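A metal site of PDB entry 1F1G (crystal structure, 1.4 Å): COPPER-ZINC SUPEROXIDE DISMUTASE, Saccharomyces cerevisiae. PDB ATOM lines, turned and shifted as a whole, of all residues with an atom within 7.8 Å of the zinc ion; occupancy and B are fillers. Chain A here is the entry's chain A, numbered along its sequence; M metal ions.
The backbone NH of His 72 lies within hydrogen-bond range of the backbone carbonyl oxygen of Leu 136 (2.9 Å). NE2 of His 72 sits at hydrogen-bond distance from OD1 of Asp 125, at 2.7 Å. O of Thr 71 is in hydrogen-bond range of N of His 81 (3.4 Å). The backbone carbonyl oxygen of Asp 84 is in hydrogen-bond range of the guanidinium group of Arg 80 (3.2 Å). The backbone carbonyl oxygen (O) of Lys 70 sits close to a ring nitrogen (NE2) of His 81, 3.1 Å away. ND1 of His 47 sits close to NE2 of His 64 (3.2 Å). N of Gly 73 sits at hydrogen-bond distance from OD2 of Asp 84 (2.9 Å).
Of the 27 residues printed, 4 come within 4 Å of the zinc ion. The nearest printed residue that does not touch the zinc ion is Lys 137 (4.02 Å).
The zinc ion is bound by the side-chain carboxylate of Asp 84 (1.9 Å), a ring nitrogen (ND1) of His 64 (2.0 Å), a ring nitrogen (ND1) of His 72 (2.0 Å) and a ring nitrogen (ND1) of His 81 (2.0 Å).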
ATOM      1  N   PHE A  46       6.118  29.514 -22.213  1.00  0.00           N
ATOM      2  CA  PHE A  46       4.948  29.342 -21.362  1.00  0.00           C
ATOM      3  C   PHE A  46       4.240  28.060 -21.809  1.00  0.00           C
ATOM      4  O   PHE A  46       3.811  27.984 -22.977  1.00  0.00           O
ATOM      5  CB  PHE A  46       4.074  30.559 -21.542  1.00  0.00           C
ATOM      6  CG  PHE A  46       2.865  30.711 -20.672  1.00  0.00           C
ATOM      7  CD1 PHE A  46       2.921  30.569 -19.315  1.00  0.00           C
ATOM      8  CD2 PHE A  46       1.640  31.041 -21.286  1.00  0.00           C
ATOM      9  CE1 PHE A  46       1.799  30.739 -18.500  1.00  0.00           C
ATOM     10  CE2 PHE A  46       0.542  31.237 -20.495  1.00  0.00           C
ATOM     11  CZ  PHE A  46       0.611  31.091 -19.133  1.00  0.00           C
ATOM     12  N   HIS A  47       4.196  27.019 -20.944  1.00  0.00           N
ATOM     13  CA  HIS A  47       3.634  25.748 -21.418  1.00  0.00           C
ATOM     14  C   HIS A  47       2.901  25.022 -20.299  1.00  0.00           C
ATOM     15  O   HIS A  47       3.163  25.174 -19.126  1.00  0.00           O
ATOM     16  CB  HIS A  47       4.672  24.735 -21.936  1.00  0.00           C
ATOM     17  CG  HIS A  47       5.840  25.368 -22.634  1.00  0.00           C
ATOM     18  ND1 HIS A  47       7.028  25.501 -21.986  1.00  0.00           N
ATOM     19  CD2 HIS A  47       5.962  25.933 -23.853  1.00  0.00           C
ATOM     20  CE1 HIS A  47       7.835  26.112 -22.823  1.00  0.00           C
ATOM     21  NE2 HIS A  47       7.262  26.406 -23.969  1.00  0.00           N
ATOM     22  N   ILE A  48       2.009  24.126 -20.752  1.00  0.00           N
ATOM     23  CA  ILE A  48       1.448  23.113 -19.877  1.00  0.00           C
ATOM     24  C   ILE A  48       2.376  21.898 -19.888  1.00  0.00           C
ATOM     25  O   ILE A  48       2.692  21.392 -20.955  1.00  0.00           O
ATOM     26  CB  ILE A  48       0.016  22.728 -20.311  1.00  0.00           C
ATOM     27  CG1 ILE A  48      -0.845  23.979 -20.455  1.00  0.00           C
ATOM     28  CG2 ILE A  48      -0.553  21.712 -19.351  1.00  0.00           C
ATOM     29  CD1 ILE A  48      -2.294  23.825 -20.834  1.00  0.00           C
ATOM     30  N   HIS A  49       2.795  21.500 -18.699  1.00  0.00           N
ATOM     31  CA  HIS A  49       3.638  20.306 -18.567  1.00  0.00           C
ATOM     32  C   HIS A  49       2.778  19.146 -18.077  1.00  0.00           C
ATOM     33  O   HIS A  49       1.677  19.301 -17.566  1.00  0.00           O
ATOM     34  CB  HIS A  49       4.804  20.630 -17.626  1.00  0.00           C
ATOM     35  CG  HIS A  49       5.832  21.505 -18.242  1.00  0.00           C
ATOM     36  ND1 HIS A  49       7.158  21.143 -18.358  1.00  0.00           N
ATOM     37  CD2 HIS A  49       5.771  22.741 -18.818  1.00  0.00           C
ATOM     38  CE1 HIS A  49       7.823  22.133 -18.937  1.00  0.00           C
ATOM     39  NE2 HIS A  49       7.032  23.123 -19.263  1.00  0.00           N
ATOM     40  N   PRO A  63       7.886  16.842 -18.668  1.00  0.00           N
ATOM     41  CA  PRO A  63       8.016  17.514 -19.949  1.00  0.00           C
ATOM     42  C   PRO A  63       6.750  18.226 -20.410  1.00  0.00           C
ATOM     43  O   PRO A  63       5.745  18.185 -19.716  1.00  0.00           O
ATOM     44  CB  PRO A  63       8.334  16.316 -20.881  1.00  0.00           C
ATOM     45  CG  PRO A  63       7.468  15.236 -20.309  1.00  0.00           C
ATOM     46  CD  PRO A  63       7.598  15.393 -18.817  1.00  0.00           C
ATOM     47  N   HIS A  64       6.797  18.877 -21.568  1.00  0.00           N
ATOM     48  CA  HIS A  64       5.594  19.494 -22.123  1.00  0.00           C
ATOM     49  C   HIS A  64       4.511  18.425 -22.296  1.00  0.00           C
ATOM     50  O   HIS A  64       4.811  17.299 -22.714  1.00  0.00           O
ATOM     51  CB  HIS A  64       5.860  20.141 -23.478  1.00  0.00           C
ATOM     52  CG  HIS A  64       6.879  21.248 -23.421  1.00  0.00           C
ATOM     53  ND1 HIS A  64       7.158  22.095 -24.443  1.00  0.00           N
ATOM     54  CD2 HIS A  64       7.663  21.641 -22.359  1.00  0.00           C
ATOM     55  CE1 HIS A  64       8.099  22.967 -24.099  1.00  0.00           C
ATOM     56  NE2 HIS A  64       8.402  22.681 -22.825  1.00  0.00           N
ATOM     57  N   PHE A  65       3.278  18.763 -21.985  1.00  0.00           N
ATOM     58  CA  PHE A  65       2.157  17.854 -22.184  1.00  0.00           C
ATOM     59  C   PHE A  65       1.983  17.586 -23.666  1.00  0.00           C
ATOM     60  O   PHE A  65       1.803  18.497 -24.468  1.00  0.00           O
ATOM     61  CB  PHE A  65       0.909  18.491 -21.557  1.00  0.00           C
ATOM     62  CG  PHE A  65      -0.318  17.593 -21.671  1.00  0.00           C
ATOM     63  CD1 PHE A  65      -0.251  16.240 -21.393  1.00  0.00           C
ATOM     64  CD2 PHE A  65      -1.529  18.150 -22.080  1.00  0.00           C
ATOM     65  CE1 PHE A  65      -1.371  15.444 -21.529  1.00  0.00           C
ATOM     66  CE2 PHE A  65      -2.665  17.358 -22.190  1.00  0.00           C
ATOM     67  CZ  PHE A  65      -2.582  16.013 -21.888  1.00  0.00           C
ATOM     68  N   ASN A  66       2.124  16.294 -24.013  1.00  0.00           N
ATOM     69  CA  ASN A  66       2.244  15.888 -25.425  1.00  0.00           C
ATOM     70  C   ASN A  66       1.622  14.534 -25.696  1.00  0.00           C
ATOM     71  O   ASN A  66       2.275  13.562 -26.128  1.00  0.00           O
ATOM     72  CB  ASN A  66       3.744  15.872 -25.791  1.00  0.00           C
ATOM     73  CG  ASN A  66       3.960  15.596 -27.259  1.00  0.00           C
ATOM     74  OD1 ASN A  66       3.156  15.921 -28.133  1.00  0.00           O
ATOM     75  ND2 ASN A  66       5.189  15.138 -27.567  1.00  0.00           N
ATOM     76  N   LYS A  70       3.906  14.719 -30.696  1.00  0.00           N
ATOM     77  CA  LYS A  70       4.312  15.650 -31.720  1.00  0.00           C
ATOM     78  C   LYS A  70       5.592  16.376 -31.269  1.00  0.00           C
ATOM     79  O   LYS A  70       5.937  16.265 -30.079  1.00  0.00           O
ATOM     80  CB  LYS A  70       3.199  16.674 -31.994  1.00  0.00           C
ATOM     81  CG  LYS A  70       1.880  16.056 -32.511  1.00  0.00           C
ATOM     82  CD  LYS A  70       0.789  17.102 -32.678  1.00  0.00           C
ATOM     83  CE  LYS A  70      -0.545  16.662 -33.208  1.00  0.00           C
ATOM     84  NZ  LYS A  70      -1.764  17.202 -32.479  1.00  0.00           N
ATOM     85  N   THR A  71       6.185  17.090 -32.207  1.00  0.00           N
ATOM     86  CA  THR A  71       7.294  17.957 -31.814  1.00  0.00           C
ATOM     87  C   THR A  71       6.767  19.283 -31.260  1.00  0.00           C
ATOM     88  O   THR A  71       5.637  19.692 -31.472  1.00  0.00           O
ATOM     89  CB  THR A  71       8.261  18.232 -32.969  1.00  0.00           C
ATOM     90  OG1 THR A  71       7.551  18.657 -34.128  1.00  0.00           O
ATOM     91  CG2 THR A  71       9.031  16.964 -33.332  1.00  0.00           C
ATOM     92  N   HIS A  72       7.687  19.942 -30.533  1.00  0.00           N
ATOM     93  CA  HIS A  72       7.432  21.254 -29.985  1.00  0.00           C
ATOM     94  C   HIS A  72       7.221  22.304 -31.065  1.00  0.00           C
ATOM     95  O   HIS A  72       8.004  22.352 -32.040  1.00  0.00           O
ATOM     96  CB  HIS A  72       8.654  21.614 -29.104  1.00  0.00           C
ATOM     97  CG  HIS A  72       8.442  22.949 -28.443  1.00  0.00           C
ATOM     98  ND1 HIS A  72       7.619  23.138 -27.345  1.00  0.00           N
ATOM     99  CD2 HIS A  72       8.967  24.154 -28.813  1.00  0.00           C
ATOM    100  CE1 HIS A  72       7.670  24.451 -27.080  1.00  0.00           C
ATOM    101  NE2 HIS A  72       8.485  25.094 -27.935  1.00  0.00           N
ATOM    102  N   GLY A  73       6.209  23.170 -30.885  1.00  0.00           N
ATOM    103  CA  GLY A  73       5.979  24.196 -31.887  1.00  0.00           C
ATOM    104  C   GLY A  73       5.365  25.464 -31.286  1.00  0.00           C
ATOM    105  O   GLY A  73       5.286  25.606 -30.086  1.00  0.00           O
ATOM    106  N   ALA A  74       4.952  26.377 -32.154  1.00  0.00           N
ATOM    107  CA  ALA A  74       4.221  27.575 -31.801  1.00  0.00           C
ATOM    108  C   ALA A  74       2.757  27.204 -31.622  1.00  0.00           C
ATOM    109  O   ALA A  74       2.266  26.250 -32.216  1.00  0.00           O
ATOM    110  CB  ALA A  74       4.313  28.618 -32.903  1.00  0.00           C
ATOM    111  N   ARG A  80       2.439  20.729 -32.917  1.00  0.00           N
ATOM    112  CA  ARG A  80       2.873  21.305 -31.651  1.00  0.00           C
ATOM    113  C   ARG A  80       2.502  20.333 -30.540  1.00  0.00           C
ATOM    114  O   ARG A  80       1.697  19.437 -30.763  1.00  0.00           O
ATOM    115  CB  ARG A  80       2.221  22.664 -31.347  1.00  0.00           C
ATOM    116  CG  ARG A  80       0.686  22.508 -31.360  1.00  0.00           C
ATOM    117  CD  ARG A  80      -0.039  23.802 -31.014  1.00  0.00           C
ATOM    118  NE  ARG A  80      -0.454  23.748 -29.642  1.00  0.00           N
ATOM    119  CZ  ARG A  80      -1.413  24.449 -29.051  1.00  0.00           C
ATOM    120  NH1 ARG A  80      -2.065  25.330 -29.781  1.00  0.00           N
ATOM    121  NH2 ARG A  80      -1.640  24.229 -27.750  1.00  0.00           N
ATOM    122  N   HIS A  81       3.067  20.492 -29.360  1.00  0.00           N
ATOM    123  CA  HIS A  81       2.579  19.828 -28.181  1.00  0.00           C
ATOM    124  C   HIS A  81       1.237  20.424 -27.730  1.00  0.00           C
ATOM    125  O   HIS A  81       1.026  21.614 -27.890  1.00  0.00           O
ATOM    126  CB  HIS A  81       3.543  20.012 -27.005  1.00  0.00           C
ATOM    127  CG  HIS A  81       4.913  19.455 -27.287  1.00  0.00           C
ATOM    128  ND1 HIS A  81       6.073  20.031 -26.770  1.00  0.00           N
ATOM    129  CD2 HIS A  81       5.339  18.419 -28.022  1.00  0.00           C
ATOM    130  CE1 HIS A  81       7.127  19.362 -27.149  1.00  0.00           C
ATOM    131  NE2 HIS A  81       6.689  18.346 -27.915  1.00  0.00           N
ATOM    132  N   VAL A  82       0.357  19.587 -27.192  1.00  0.00           N
ATOM    133  CA  VAL A  82      -0.875  20.188 -26.636  1.00  0.00           C
ATOM    134  C   VAL A  82      -0.556  21.318 -25.668  1.00  0.00           C
ATOM    135  O   VAL A  82      -1.206  22.360 -25.678  1.00  0.00           O
ATOM    136  CB  VAL A  82      -1.697  19.136 -25.887  1.00  0.00           C
ATOM    137  CG1 VAL A  82      -2.775  19.806 -25.017  1.00  0.00           C
ATOM    138  CG2 VAL A  82      -2.349  18.183 -26.872  1.00  0.00           C
ATOM    139  N   GLY A  83       0.500  21.152 -24.847  1.00  0.00           N
ATOM    140  CA  GLY A  83       0.765  22.184 -23.853  1.00  0.00           C
ATOM    141  C   GLY A  83       1.491  23.413 -24.391  1.00  0.00           C
ATOM    142  O   GLY A  83       1.745  24.283 -23.534  1.00  0.00           O
ATOM    143  N   ASP A  84       1.817  23.567 -25.655  1.00  0.00           N
ATOM    144  CA  ASP A  84       2.630  24.684 -26.135  1.00  0.00           C
ATOM    145  C   ASP A  84       1.815  25.977 -26.181  1.00  0.00           C
ATOM    146  O   ASP A  84       0.871  26.119 -26.963  1.00  0.00           O
ATOM    147  CB  ASP A  84       3.216  24.356 -27.505  1.00  0.00           C
ATOM    148  CG  ASP A  84       4.314  23.310 -27.400  1.00  0.00           C
ATOM    149  OD1 ASP A  84       4.820  23.086 -26.294  1.00  0.00           O
ATOM    150  OD2 ASP A  84       4.626  22.724 -28.455  1.00  0.00           O
ATOM    151  N   MET A  85       2.186  26.954 -25.346  1.00  0.00           N
ATOM    152  CA  MET A  85       1.515  28.236 -25.305  1.00  0.00           C
ATOM    153  C   MET A  85       2.461  29.370 -25.731  1.00  0.00           C
ATOM    154  O   MET A  85       2.146  30.522 -25.508  1.00  0.00           O
ATOM    155  CB  MET A  85       0.875  28.554 -23.925  1.00  0.00           C
ATOM    156  CG  MET A  85      -0.088  27.432 -23.508  1.00  0.00           C
ATOM    157  SD  MET A  85      -0.976  27.818 -21.969  1.00  0.00           S
ATOM    158  CE  MET A  85       0.384  27.686 -20.782  1.00  0.00           C
ATOM    159  N   GLY A  86       3.558  29.024 -26.402  1.00  0.00           N
ATOM    160  CA  GLY A  86       4.437  29.979 -26.998  1.00  0.00           C
ATOM    161  C   GLY A  86       5.164  30.876 -26.007  1.00  0.00           C
ATOM    162  O   GLY A  86       5.574  30.412 -24.930  1.00  0.00           O
ATOM    163  N   ASP A 125      11.139  30.954 -25.834  1.00  0.00           N
ATOM    164  CA  ASP A 125      10.846  29.729 -26.583  1.00  0.00           C
ATOM    165  C   ASP A 125      11.126  29.950 -28.054  1.00  0.00           C
ATOM    166  O   ASP A 125      10.568  30.876 -28.620  1.00  0.00           O
ATOM    167  CB  ASP A 125       9.367  29.410 -26.326  1.00  0.00           C
ATOM    168  CG  ASP A 125       8.817  28.141 -26.917  1.00  0.00           C
ATOM    169  OD1 ASP A 125       9.376  27.654 -27.911  1.00  0.00           O
ATOM    170  OD2 ASP A 125       7.795  27.658 -26.395  1.00  0.00           O
ATOM    171  N   GLY A 128      10.352  25.750 -31.723  1.00  0.00           N
ATOM    172  CA  GLY A 128      10.666  24.560 -32.551  1.00  0.00           C
ATOM    173  C   GLY A 128      11.465  24.888 -33.779  1.00  0.00           C
ATOM    174  O   GLY A 128      11.692  24.017 -34.652  1.00  0.00           O
ATOM    175  N   SER A 135      15.439  22.046 -29.678  1.00  0.00           N
ATOM    176  CA  SER A 135      14.360  22.953 -30.092  1.00  0.00           C
ATOM    177  C   SER A 135      13.039  22.217 -30.248  1.00  0.00           C
ATOM    178  O   SER A 135      11.975  22.692 -29.867  1.00  0.00           O
ATOM    179  CB  SER A 135      14.751  23.633 -31.400  1.00  0.00           C
ATOM    180  OG  SER A 135      13.715  24.473 -31.879  1.00  0.00           O
ATOM    181  N   LEU A 136      13.108  21.000 -30.812  1.00  0.00           N
ATOM    182  CA  LEU A 136      11.912  20.197 -31.042  1.00  0.00           C
ATOM    183  C   LEU A 136      11.358  19.574 -29.775  1.00  0.00           C
ATOM    184  O   LEU A 136      10.305  18.928 -29.808  1.00  0.00           O
ATOM    185  CB  LEU A 136      12.245  19.097 -32.065  1.00  0.00           C
ATOM    186  CG  LEU A 136      12.626  19.620 -33.448  1.00  0.00           C
ATOM    187  CD1 LEU A 136      13.112  18.511 -34.361  1.00  0.00           C
ATOM    188  CD2 LEU A 136      11.416  20.345 -34.049  1.00  0.00           C
ATOM    189  N   LYS A 137      12.028  19.713 -28.624  1.00  0.00           N
ATOM    190  CA  LYS A 137      11.607  19.124 -27.374  1.00  0.00           C
ATOM    191  C   LYS A 137      11.051  20.205 -26.418  1.00  0.00           C
ATOM    192  O   LYS A 137       9.941  20.076 -25.889  1.00  0.00           O
ATOM    193  CB  LYS A 137      12.703  18.299 -26.710  1.00  0.00           C
ATOM    194  CG  LYS A 137      13.016  17.006 -27.442  1.00  0.00           C
ATOM    195  CD  LYS A 137      13.254  17.009 -28.923  1.00  0.00           C
ATOM    196  CE  LYS A 137      14.488  16.276 -29.373  1.00  0.00           C
ATOM    197  NZ  LYS A 137      14.661  16.296 -30.856  1.00  0.00           N
ATOM    198  N   THR A 138      11.847  21.255 -26.244  1.00  0.00           N
ATOM    199  CA  THR A 138      11.546  22.286 -25.278  1.00  0.00           C
ATOM    200  C   THR A 138      11.474  23.689 -25.842  1.00  0.00           C
ATOM    201  O   THR A 138      11.204  24.625 -25.098  1.00  0.00           O
ATOM    202  CB  THR A 138      12.654  22.347 -24.187  1.00  0.00           C
ATOM    203  OG1 THR A 138      13.860  22.711 -24.859  1.00  0.00           O
ATOM    204  CG2 THR A 138      12.842  20.983 -23.526  1.00  0.00           C
ATOM    205  N   GLY A 139      11.790  23.884 -27.111  1.00  0.00           N
ATOM    206  CA  GLY A 139      11.936  25.233 -27.631  1.00  0.00           C
ATOM    207  C   GLY A 139      13.123  25.975 -27.038  1.00  0.00           C
ATOM    208  O   GLY A 139      13.246  27.176 -27.270  1.00  0.00           O
HETATM  209 ZN    ZN M   1       6.413  21.967 -26.278  1.00  0.00          ZN
HETATM  210 CU    CU M   2       7.517  24.692 -20.285  1.00  0.00          CU
